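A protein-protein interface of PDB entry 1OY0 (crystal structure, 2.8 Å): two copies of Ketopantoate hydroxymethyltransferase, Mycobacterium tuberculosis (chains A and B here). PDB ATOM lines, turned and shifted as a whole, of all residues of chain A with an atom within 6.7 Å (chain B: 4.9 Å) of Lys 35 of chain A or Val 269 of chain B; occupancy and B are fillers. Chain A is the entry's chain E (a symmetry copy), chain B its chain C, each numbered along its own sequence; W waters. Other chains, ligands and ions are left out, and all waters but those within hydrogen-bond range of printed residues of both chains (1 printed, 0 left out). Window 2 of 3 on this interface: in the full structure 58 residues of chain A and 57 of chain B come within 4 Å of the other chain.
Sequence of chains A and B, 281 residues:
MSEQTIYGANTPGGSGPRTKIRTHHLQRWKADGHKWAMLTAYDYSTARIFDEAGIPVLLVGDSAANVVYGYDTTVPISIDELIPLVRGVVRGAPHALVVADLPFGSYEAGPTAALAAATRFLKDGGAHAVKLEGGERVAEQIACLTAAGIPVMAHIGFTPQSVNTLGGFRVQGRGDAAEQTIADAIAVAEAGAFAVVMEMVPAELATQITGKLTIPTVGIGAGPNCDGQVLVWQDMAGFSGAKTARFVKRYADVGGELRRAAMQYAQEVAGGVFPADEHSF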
ATOM      1  N   TRP A  29     -10.464 -25.906  -4.966  1.00  0.00           N
ATOM      2  CA  TRP A  29     -10.429 -24.456  -4.936  1.00  0.00           C
ATOM      3  C   TRP A  29      -9.537 -23.840  -6.015  1.00  0.00           C
ATOM      4  O   TRP A  29      -9.832 -22.758  -6.526  1.00  0.00           O
ATOM      5  CB  TRP A  29      -9.993 -23.967  -3.555  1.00  0.00           C
ATOM      6  CG  TRP A  29     -11.016 -24.228  -2.494  1.00  0.00           C
ATOM      7  CD1 TRP A  29     -12.346 -24.472  -2.679  1.00  0.00           C
ATOM      8  CD2 TRP A  29     -10.802 -24.232  -1.077  1.00  0.00           C
ATOM      9  NE1 TRP A  29     -12.974 -24.628  -1.467  1.00  0.00           N
ATOM     10  CE2 TRP A  29     -12.051 -24.486  -0.466  1.00  0.00           C
ATOM     11  CE3 TRP A  29      -9.678 -24.047  -0.263  1.00  0.00           C
ATOM     12  CZ2 TRP A  29     -12.207 -24.562   0.925  1.00  0.00           C
ATOM     13  CZ3 TRP A  29      -9.833 -24.123   1.119  1.00  0.00           C
ATOM     14  CH2 TRP A  29     -11.089 -24.379   1.697  1.00  0.00           C
ATOM     15  N   ASP A  32     -11.836 -24.054  -9.003  1.00  0.00           N
ATOM     16  CA  ASP A  32     -12.915 -23.080  -8.946  1.00  0.00           C
ATOM     17  C   ASP A  32     -12.402 -21.647  -8.847  1.00  0.00           C
ATOM     18  O   ASP A  32     -13.188 -20.700  -8.850  1.00  0.00           O
ATOM     19  CB  ASP A  32     -13.838 -23.379  -7.765  1.00  0.00           C
ATOM     20  CG  ASP A  32     -14.379 -24.808  -7.793  1.00  0.00           C
ATOM     21  OD1 ASP A  32     -14.629 -25.328  -8.908  1.00  0.00           O
ATOM     22  OD2 ASP A  32     -14.561 -25.410  -6.705  1.00  0.00           O
ATOM     23  N   GLY A  33     -11.086 -21.488  -8.765  1.00  0.00           N
ATOM     24  CA  GLY A  33     -10.518 -20.155  -8.663  1.00  0.00           C
ATOM     25  C   GLY A  33     -10.729 -19.489  -7.308  1.00  0.00           C
ATOM     26  O   GLY A  33     -10.663 -18.265  -7.191  1.00  0.00           O
ATOM     27  N   HIS A  34     -10.980 -20.294  -6.282  1.00  0.00           N
ATOM     28  CA  HIS A  34     -11.191 -19.778  -4.934  1.00  0.00           C
ATOM     29  C   HIS A  34      -9.857 -19.565  -4.216  1.00  0.00           C
ATOM     30  O   HIS A  34      -9.116 -20.523  -3.951  1.00  0.00           O
ATOM     31  CB  HIS A  34     -12.052 -20.750  -4.135  1.00  0.00           C
ATOM     32  CG  HIS A  34     -12.383 -20.261  -2.765  1.00  0.00           C
ATOM     33  ND1 HIS A  34     -12.783 -18.965  -2.523  1.00  0.00           N
ATOM     34  CD2 HIS A  34     -12.411 -20.895  -1.568  1.00  0.00           C
ATOM     35  CE1 HIS A  34     -13.045 -18.821  -1.235  1.00  0.00           C
ATOM     36  NE2 HIS A  34     -12.827 -19.977  -0.633  1.00  0.00           N
ATOM     37  N   LYS A  35      -9.550 -18.307  -3.917  1.00  0.00           N
ATOM     38  CA  LYS A  35      -8.306 -17.967  -3.230  1.00  0.00           C
ATOM     39  C   LYS A  35      -8.521 -18.110  -1.720  1.00  0.00           C
ATOM     40  O   LYS A  35      -9.263 -17.338  -1.118  1.00  0.00           O
ATOM     41  CB  LYS A  35      -7.894 -16.537  -3.588  1.00  0.00           C
ATOM     42  CG  LYS A  35      -7.782 -16.318  -5.088  1.00  0.00           C
ATOM     43  CD  LYS A  35      -8.019 -14.861  -5.453  1.00  0.00           C
ATOM     44  CE  LYS A  35      -8.202 -14.689  -6.963  1.00  0.00           C
ATOM     45  NZ  LYS A  35      -8.618 -13.294  -7.335  1.00  0.00           N
ATOM     46  N   TRP A  36      -7.873 -19.112  -1.124  1.00  0.00           N
ATOM     47  CA  TRP A  36      -8.001 -19.386   0.304  1.00  0.00           C
ATOM     48  C   TRP A  36      -6.867 -18.787   1.134  1.00  0.00           C
ATOM     49  O   TRP A  36      -5.766 -18.527   0.632  1.00  0.00           O
ATOM     50  CB  TRP A  36      -8.087 -20.900   0.549  1.00  0.00           C
ATOM     51  CG  TRP A  36      -7.009 -21.704  -0.126  1.00  0.00           C
ATOM     52  CD1 TRP A  36      -6.953 -22.059  -1.441  1.00  0.00           C
ATOM     53  CD2 TRP A  36      -5.827 -22.235   0.484  1.00  0.00           C
ATOM     54  NE1 TRP A  36      -5.807 -22.779  -1.694  1.00  0.00           N
ATOM     55  CE2 TRP A  36      -5.099 -22.903  -0.529  1.00  0.00           C
ATOM     56  CE3 TRP A  36      -5.310 -22.212   1.787  1.00  0.00           C
ATOM     57  CZ2 TRP A  36      -3.884 -23.543  -0.278  1.00  0.00           C
ATOM     58  CZ3 TRP A  36      -4.102 -22.846   2.034  1.00  0.00           C
ATOM     59  CH2 TRP A  36      -3.403 -23.504   1.005  1.00  0.00           C
ATOM     60  N   ALA A  37      -7.155 -18.581   2.412  1.00  0.00           N
ATOM     61  CA  ALA A  37      -6.195 -17.989   3.332  1.00  0.00           C
ATOM     62  C   ALA A  37      -5.643 -18.973   4.354  1.00  0.00           C
ATOM     63  O   ALA A  37      -6.386 -19.759   4.952  1.00  0.00           O
ATOM     64  CB  ALA A  37      -6.841 -16.801   4.052  1.00  0.00           C
ATOM     65  N   MET A  38      -4.329 -18.920   4.544  1.00  0.00           N
ATOM     66  CA  MET A  38      -3.654 -19.781   5.503  1.00  0.00           C
ATOM     67  C   MET A  38      -3.027 -18.905   6.572  1.00  0.00           C
ATOM     68  O   MET A  38      -2.372 -17.899   6.283  1.00  0.00           O
ATOM     69  CB  MET A  38      -2.571 -20.618   4.819  1.00  0.00           C
ATOM     70  CG  MET A  38      -1.766 -21.490   5.777  1.00  0.00           C
ATOM     71  SD  MET A  38      -0.837 -22.798   4.940  1.00  0.00           S
ATOM     72  CE  MET A  38       0.678 -21.973   4.518  1.00  0.00           C
ATOM     73  N   PRO A 224       0.041 -11.261  -5.638  1.00  0.00           N
ATOM     74  CA  PRO A 224      -1.377 -11.630  -5.544  1.00  0.00           C
ATOM     75  C   PRO A 224      -1.771 -12.831  -6.394  1.00  0.00           C
ATOM     76  O   PRO A 224      -2.863 -13.375  -6.240  1.00  0.00           O
ATOM     77  CB  PRO A 224      -2.079 -10.358  -6.007  1.00  0.00           C
ATOM     78  CG  PRO A 224      -1.180  -9.918  -7.132  1.00  0.00           C
ATOM     79  CD  PRO A 224       0.217 -10.102  -6.540  1.00  0.00           C
ATOM     80  N   CYS A 226      -1.422 -16.133  -6.551  1.00  0.00           N
ATOM     81  CA  CYS A 226      -1.157 -17.411  -5.919  1.00  0.00           C
ATOM     82  C   CYS A 226      -2.514 -17.966  -5.519  1.00  0.00           C
ATOM     83  O   CYS A 226      -3.403 -17.209  -5.114  1.00  0.00           O
ATOM     84  CB  CYS A 226      -0.278 -17.213  -4.680  1.00  0.00           C
ATOM     85  SG  CYS A 226       1.308 -16.416  -5.036  1.00  0.00           S
ATOM     86  N   ASP A 227      -2.679 -19.278  -5.642  1.00  0.00           N
ATOM     87  CA  ASP A 227      -3.940 -19.930  -5.295  1.00  0.00           C
ATOM     88  C   ASP A 227      -4.384 -19.653  -3.854  1.00  0.00           C
ATOM     89  O   ASP A 227      -5.568 -19.767  -3.520  1.00  0.00           O
ATOM     90  CB  ASP A 227      -3.805 -21.430  -5.531  1.00  0.00           C
ATOM     91  CG  ASP A 227      -3.378 -21.743  -6.948  1.00  0.00           C
ATOM     92  OD1 ASP A 227      -4.205 -21.550  -7.867  1.00  0.00           O
ATOM     93  OD2 ASP A 227      -2.211 -22.155  -7.154  1.00  0.00           O
ATOM     94  N   GLY A 228      -3.425 -19.287  -3.008  1.00  0.00           N
ATOM     95  CA  GLY A 228      -3.717 -18.982  -1.617  1.00  0.00           C
ATOM     96  C   GLY A 228      -2.644 -18.093  -1.007  1.00  0.00           C
ATOM     97  O   GLY A 228      -1.573 -17.898  -1.591  1.00  0.00           O
ATOM     98  N   GLN A 229      -2.927 -17.554   0.173  1.00  0.00           N
ATOM     99  CA  GLN A 229      -1.981 -16.679   0.860  1.00  0.00           C
ATOM    100  C   GLN A 229      -1.706 -17.165   2.281  1.00  0.00           C
ATOM    101  O   GLN A 229      -2.549 -17.826   2.900  1.00  0.00           O
ATOM    102  CB  GLN A 229      -2.539 -15.250   0.915  1.00  0.00           C
ATOM    103  CG  GLN A 229      -2.713 -14.614  -0.440  1.00  0.00           C
ATOM    104  CD  GLN A 229      -1.387 -14.332  -1.105  1.00  0.00           C
ATOM    105  OE1 GLN A 229      -1.284 -14.318  -2.333  1.00  0.00           O
ATOM    106  NE2 GLN A 229      -0.361 -14.093  -0.300  1.00  0.00           N
ATOM    107  N   VAL A 230      -0.527 -16.833   2.797  1.00  0.00           N
ATOM    108  CA  VAL A 230      -0.168 -17.221   4.150  1.00  0.00           C
ATOM    109  C   VAL A 230       0.613 -16.129   4.869  1.00  0.00           C
ATOM    110  O   VAL A 230       1.504 -15.501   4.298  1.00  0.00           O
ATOM    111  CB  VAL A 230       0.675 -18.500   4.163  1.00  0.00           C
ATOM    112  CG1 VAL A 230       1.999 -18.256   3.457  1.00  0.00           C
ATOM    113  CG2 VAL A 230       0.895 -18.950   5.596  1.00  0.00           C
ATOM    114  N   TYR A 251      -3.635  -6.117   9.818  1.00  0.00           N
ATOM    115  CA  TYR A 251      -5.094  -6.085   9.912  1.00  0.00           C
ATOM    116  C   TYR A 251      -5.644  -5.644  11.253  1.00  0.00           C
ATOM    117  O   TYR A 251      -6.863  -5.596  11.436  1.00  0.00           O
ATOM    118  CB  TYR A 251      -5.689  -7.454   9.577  1.00  0.00           C
ATOM    119  CG  TYR A 251      -5.680  -7.771   8.108  1.00  0.00           C
ATOM    120  CD1 TYR A 251      -4.486  -8.073   7.449  1.00  0.00           C
ATOM    121  CD2 TYR A 251      -6.866  -7.738   7.360  1.00  0.00           C
ATOM    122  CE1 TYR A 251      -4.465  -8.334   6.078  1.00  0.00           C
ATOM    123  CE2 TYR A 251      -6.861  -7.996   5.989  1.00  0.00           C
ATOM    124  CZ  TYR A 251      -5.653  -8.295   5.356  1.00  0.00           C
ATOM    125  OH  TYR A 251      -5.627  -8.558   4.006  1.00  0.00           O
ATOM    126  N   GLN B 264     -11.297 -10.861   8.049  1.00  0.00           N
ATOM    127  CA  GLN B 264     -11.088  -9.847   7.039  1.00  0.00           C
ATOM    128  C   GLN B 264      -9.937 -10.262   6.140  1.00  0.00           C
ATOM    129  O   GLN B 264     -10.014 -10.144   4.913  1.00  0.00           O
ATOM    130  CB  GLN B 264     -10.788  -8.493   7.670  1.00  0.00           C
ATOM    131  CG  GLN B 264     -11.522  -7.365   6.960  1.00  0.00           C
ATOM    132  CD  GLN B 264     -10.661  -6.133   6.801  1.00  0.00           C
ATOM    133  OE1 GLN B 264     -10.124  -5.604   7.785  1.00  0.00           O
ATOM    134  NE2 GLN B 264     -10.520  -5.662   5.557  1.00  0.00           N
ATOM    135  N   TYR B 265      -8.865 -10.746   6.756  1.00  0.00           N
ATOM    136  CA  TYR B 265      -7.702 -11.203   6.007  1.00  0.00           C
ATOM    137  C   TYR B 265      -8.151 -12.229   4.968  1.00  0.00           C
ATOM    138  O   TYR B 265      -7.804 -12.143   3.788  1.00  0.00           O
ATOM    139  CB  TYR B 265      -6.697 -11.840   6.968  1.00  0.00           C
ATOM    140  CG  TYR B 265      -5.675 -12.734   6.307  1.00  0.00           C
ATOM    141  CD1 TYR B 265      -4.694 -12.208   5.462  1.00  0.00           C
ATOM    142  CD2 TYR B 265      -5.683 -14.110   6.536  1.00  0.00           C
ATOM    143  CE1 TYR B 265      -3.739 -13.032   4.864  1.00  0.00           C
ATOM    144  CE2 TYR B 265      -4.736 -14.946   5.940  1.00  0.00           C
ATOM    145  CZ  TYR B 265      -3.767 -14.401   5.109  1.00  0.00           C
ATOM    146  OH  TYR B 265      -2.830 -15.224   4.528  1.00  0.00           O
ATOM    147  N   ALA B 266      -8.942 -13.193   5.424  1.00  0.00           N
ATOM    148  CA  ALA B 266      -9.441 -14.247   4.556  1.00  0.00           C
ATOM    149  C   ALA B 266     -10.215 -13.696   3.361  1.00  0.00           C
ATOM    150  O   ALA B 266      -9.958 -14.069   2.213  1.00  0.00           O
ATOM    151  CB  ALA B 266     -10.324 -15.200   5.358  1.00  0.00           C
ATOM    152  N   GLN B 267     -11.161 -12.804   3.632  1.00  0.00           N
ATOM    153  CA  GLN B 267     -11.976 -12.222   2.574  1.00  0.00           C
ATOM    154  C   GLN B 267     -11.150 -11.429   1.567  1.00  0.00           C
ATOM    155  O   GLN B 267     -11.372 -11.535   0.363  1.00  0.00           O
ATOM    156  CB  GLN B 267     -13.064 -11.338   3.177  1.00  0.00           C
ATOM    157  CG  GLN B 267     -14.192 -11.069   2.220  1.00  0.00           C
ATOM    158  CD  GLN B 267     -15.489 -10.760   2.939  1.00  0.00           C
ATOM    159  OE1 GLN B 267     -15.578  -9.780   3.688  1.00  0.00           O
ATOM    160  NE2 GLN B 267     -16.505 -11.597   2.722  1.00  0.00           N
ATOM    161  N   GLU B 268     -10.200 -10.643   2.056  1.00  0.00           N
ATOM    162  CA  GLU B 268      -9.351  -9.859   1.168  1.00  0.00           C
ATOM    163  C   GLU B 268      -8.538 -10.776   0.266  1.00  0.00           C
ATOM    164  O   GLU B 268      -8.268 -10.443  -0.888  1.00  0.00           O
ATOM    165  CB  GLU B 268      -8.402  -8.971   1.971  1.00  0.00           C
ATOM    166  CG  GLU B 268      -9.095  -7.901   2.791  1.00  0.00           C
ATOM    167  CD  GLU B 268      -8.162  -6.754   3.137  1.00  0.00           C
ATOM    168  OE1 GLU B 268      -8.589  -5.851   3.888  1.00  0.00           O
ATOM    169  OE2 GLU B 268      -7.005  -6.748   2.652  1.00  0.00           O
ATOM    170  N   VAL B 269      -8.143 -11.926   0.810  1.00  0.00           N
ATOM    171  CA  VAL B 269      -7.369 -12.903   0.054  1.00  0.00           C
ATOM    172  C   VAL B 269      -8.266 -13.421  -1.065  1.00  0.00           C
ATOM    173  O   VAL B 269      -7.860 -13.497  -2.234  1.00  0.00           O
ATOM    174  CB  VAL B 269      -6.937 -14.089   0.948  1.00  0.00           C
ATOM    175  CG1 VAL B 269      -6.307 -15.184   0.100  1.00  0.00           C
ATOM    176  CG2 VAL B 269      -5.953 -13.603   2.002  1.00  0.00           C
ATOM    177  N   ALA B 270      -9.492 -13.768  -0.691  1.00  0.00           N
ATOM    178  CA  ALA B 270     -10.472 -14.278  -1.635  1.00  0.00           C
ATOM    179  C   ALA B 270     -10.825 -13.197  -2.639  1.00  0.00           C
ATOM    180  O   ALA B 270     -11.065 -13.483  -3.815  1.00  0.00           O
ATOM    181  CB  ALA B 270     -11.716 -14.723  -0.901  1.00  0.00           C
ATOM    182  N   GLY B 271     -10.848 -11.953  -2.173  1.00  0.00           N
ATOM    183  CA  GLY B 271     -11.185 -10.848  -3.050  1.00  0.00           C
ATOM    184  C   GLY B 271     -10.008 -10.288  -3.826  1.00  0.00           C
ATOM    185  O   GLY B 271     -10.128  -9.244  -4.473  1.00  0.00           O
ATOM    186  N   GLY B 272      -8.870 -10.971  -3.767  1.00  0.00           N
ATOM    187  CA  GLY B 272      -7.700 -10.498  -4.482  1.00  0.00           C
ATOM    188  C   GLY B 272      -7.207  -9.140  -4.014  1.00  0.00           C
ATOM    189  O   GLY B 272      -6.245  -8.615  -4.582  1.00  0.00           O
ATOM    190  N   PHE B 274      -5.860  -8.602  -1.188  1.00  0.00           N
ATOM    191  CA  PHE B 274      -4.583  -8.910  -0.540  1.00  0.00           C
ATOM    192  C   PHE B 274      -4.002 -10.193  -1.128  1.00  0.00           C
ATOM    193  O   PHE B 274      -4.719 -11.182  -1.325  1.00  0.00           O
ATOM    194  CB  PHE B 274      -4.716  -9.106   0.972  1.00  0.00           C
ATOM    195  CG  PHE B 274      -3.401  -9.441   1.639  1.00  0.00           C
ATOM    196  CD1 PHE B 274      -2.457  -8.441   1.895  1.00  0.00           C
ATOM    197  CD2 PHE B 274      -3.059 -10.767   1.916  1.00  0.00           C
ATOM    198  CE1 PHE B 274      -1.189  -8.757   2.410  1.00  0.00           C
ATOM    199  CE2 PHE B 274      -1.800 -11.093   2.428  1.00  0.00           C
ATOM    200  CZ  PHE B 274      -0.863 -10.086   2.675  1.00  0.00           C
HETATM  201  O   HOH W   1      -9.816 -16.707   1.312  1.00  0.00           O
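The side-chain hydroxyl of Tyr 265 of chain B sits at hydrogen-bond distance from the backbone NH of Val 230 of chain A (3.3 Å).
OE2 of Glu 268 of chain B lies within hydrogen-bond range of OH of Tyr 251 of chain A, at 2.6 Å.
OH of Tyr 265 of chain B sits at hydrogen-bond distance from O of Gln 229 of chain A (3.1 Å).
The side-chain hydroxyl (OH) of Tyr 265 of chain B lies within hydrogen-bond range of the backbone carbonyl oxygen (O) of Met 38 of chain A.
The backbone NH (N) of Met 38 of chain A sits at hydrogen-bond distance from the backbone carbonyl oxygen (O) of Gln 229 of chain A, at 2.7 Å.
O of Trp 36 of chain A lies within hydrogen-bond range of N of Gln 229 of chain A.
The side-chain amide nitrogen of Gln 264 of chain B sits at hydrogen-bond distance from the side-chain carboxylate of Glu 268 of chain B (2.6 Å).
O of Asp 227 of chain A is in hydrogen-bond range of N of Trp 36 of chain A, at 3.4 Å.
N of Phe 274 of chain B sits at hydrogen-bond distance from O of Glu 268 of chain B, 3.0 Å away.
Lys 35 of chain A touches Val 269 of chain B (CB to O, 3.3 Å).
Lys 35 of chain A touches Ala 270 of chain B.
CG1 of Val 269 of chain B touches O of Trp 36 of chain A (3.4 Å).
Ala 37 of chain A touches Tyr 265 of chain B (CB to CE2, 3.4 Å).
Ala 37 of chain A touches Ala 266 of chain B.
Val 269 of chain B touches Ala 37 of chain A (CG2 to CB, 3.9 Å).
CG of Gln 229 of chain A touches CG1 of Val 269 of chain B, at 3.7 Å.
Gln 264 of chain B touches Tyr 251 of chain A (C to CE2, 3.8 Å).
Tyr 251 of chain A touches Tyr 265 of chain B (CE2 to CA, 3.3 Å).
Tyr 251 of chain A touches Phe 274 of chain B (OH to CB, 3.2 Å).
Trp 29 of chain A touches none of the printed residues of chain B.
Of the printed residues of chain B, Lys 35 of chain A touches Val 269 and Ala 270.
Of the printed residues of chain B, Ala 37 of chain A touches Tyr 265 (3.4 Å), Ala 266 (3.7 Å) and Val 269 (3.9 Å).
Pro 224 of chain A touches none of the printed residues of chain B.
Printed residues of chain B within 4 Å of Val 230 of chain A: Tyr 265 (3.3 Å).
Of the printed residues of chain A, Gln 264 of chain B touches Tyr 251.
Of the printed residues of chain A, Val 269 of chain B touches Lys 35, Trp 36, Ala 37 and Gln 229.
Of the printed residues of chain A, Ala 270 of chain B touches Lys 35.
The nearest residue of chain A that does not touch Val 269 of chain B is Gly 228 of chain A (4.8 Å).
Printed residues of chain A that touch a printed residue of chain B: Lys 35, Trp 36, Ala 37, Met 38, Gln 229, Val 230 and Tyr 251.
Hydrophobic or aromatic side chains of chain A within 4 Å of the printed part of chain B: Ala 37 and Tyr 251.
Printed residues of chain B that touch a printed residue of chain A: Gln 264, Tyr 265, Ala 266, Glu 268, Val 269, Ala 270 and Phe 274.
Among the printed residues, 14 pairs touch across the chains.
Among the printed residues, no Asp or Glu carboxylate lies within 4 Å of a Lys or Arg side-chain nitrogen of the other chain.
No position is printed for both chains.
Water W1 lies within hydrogen-bond range of the backbone carbonyl oxygen (O) of Lys 35 of chain A, the backbone carbonyl oxygen (O) of Ala 266 of chain B and the backbone NH (N) of Ala 37 of chain A.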
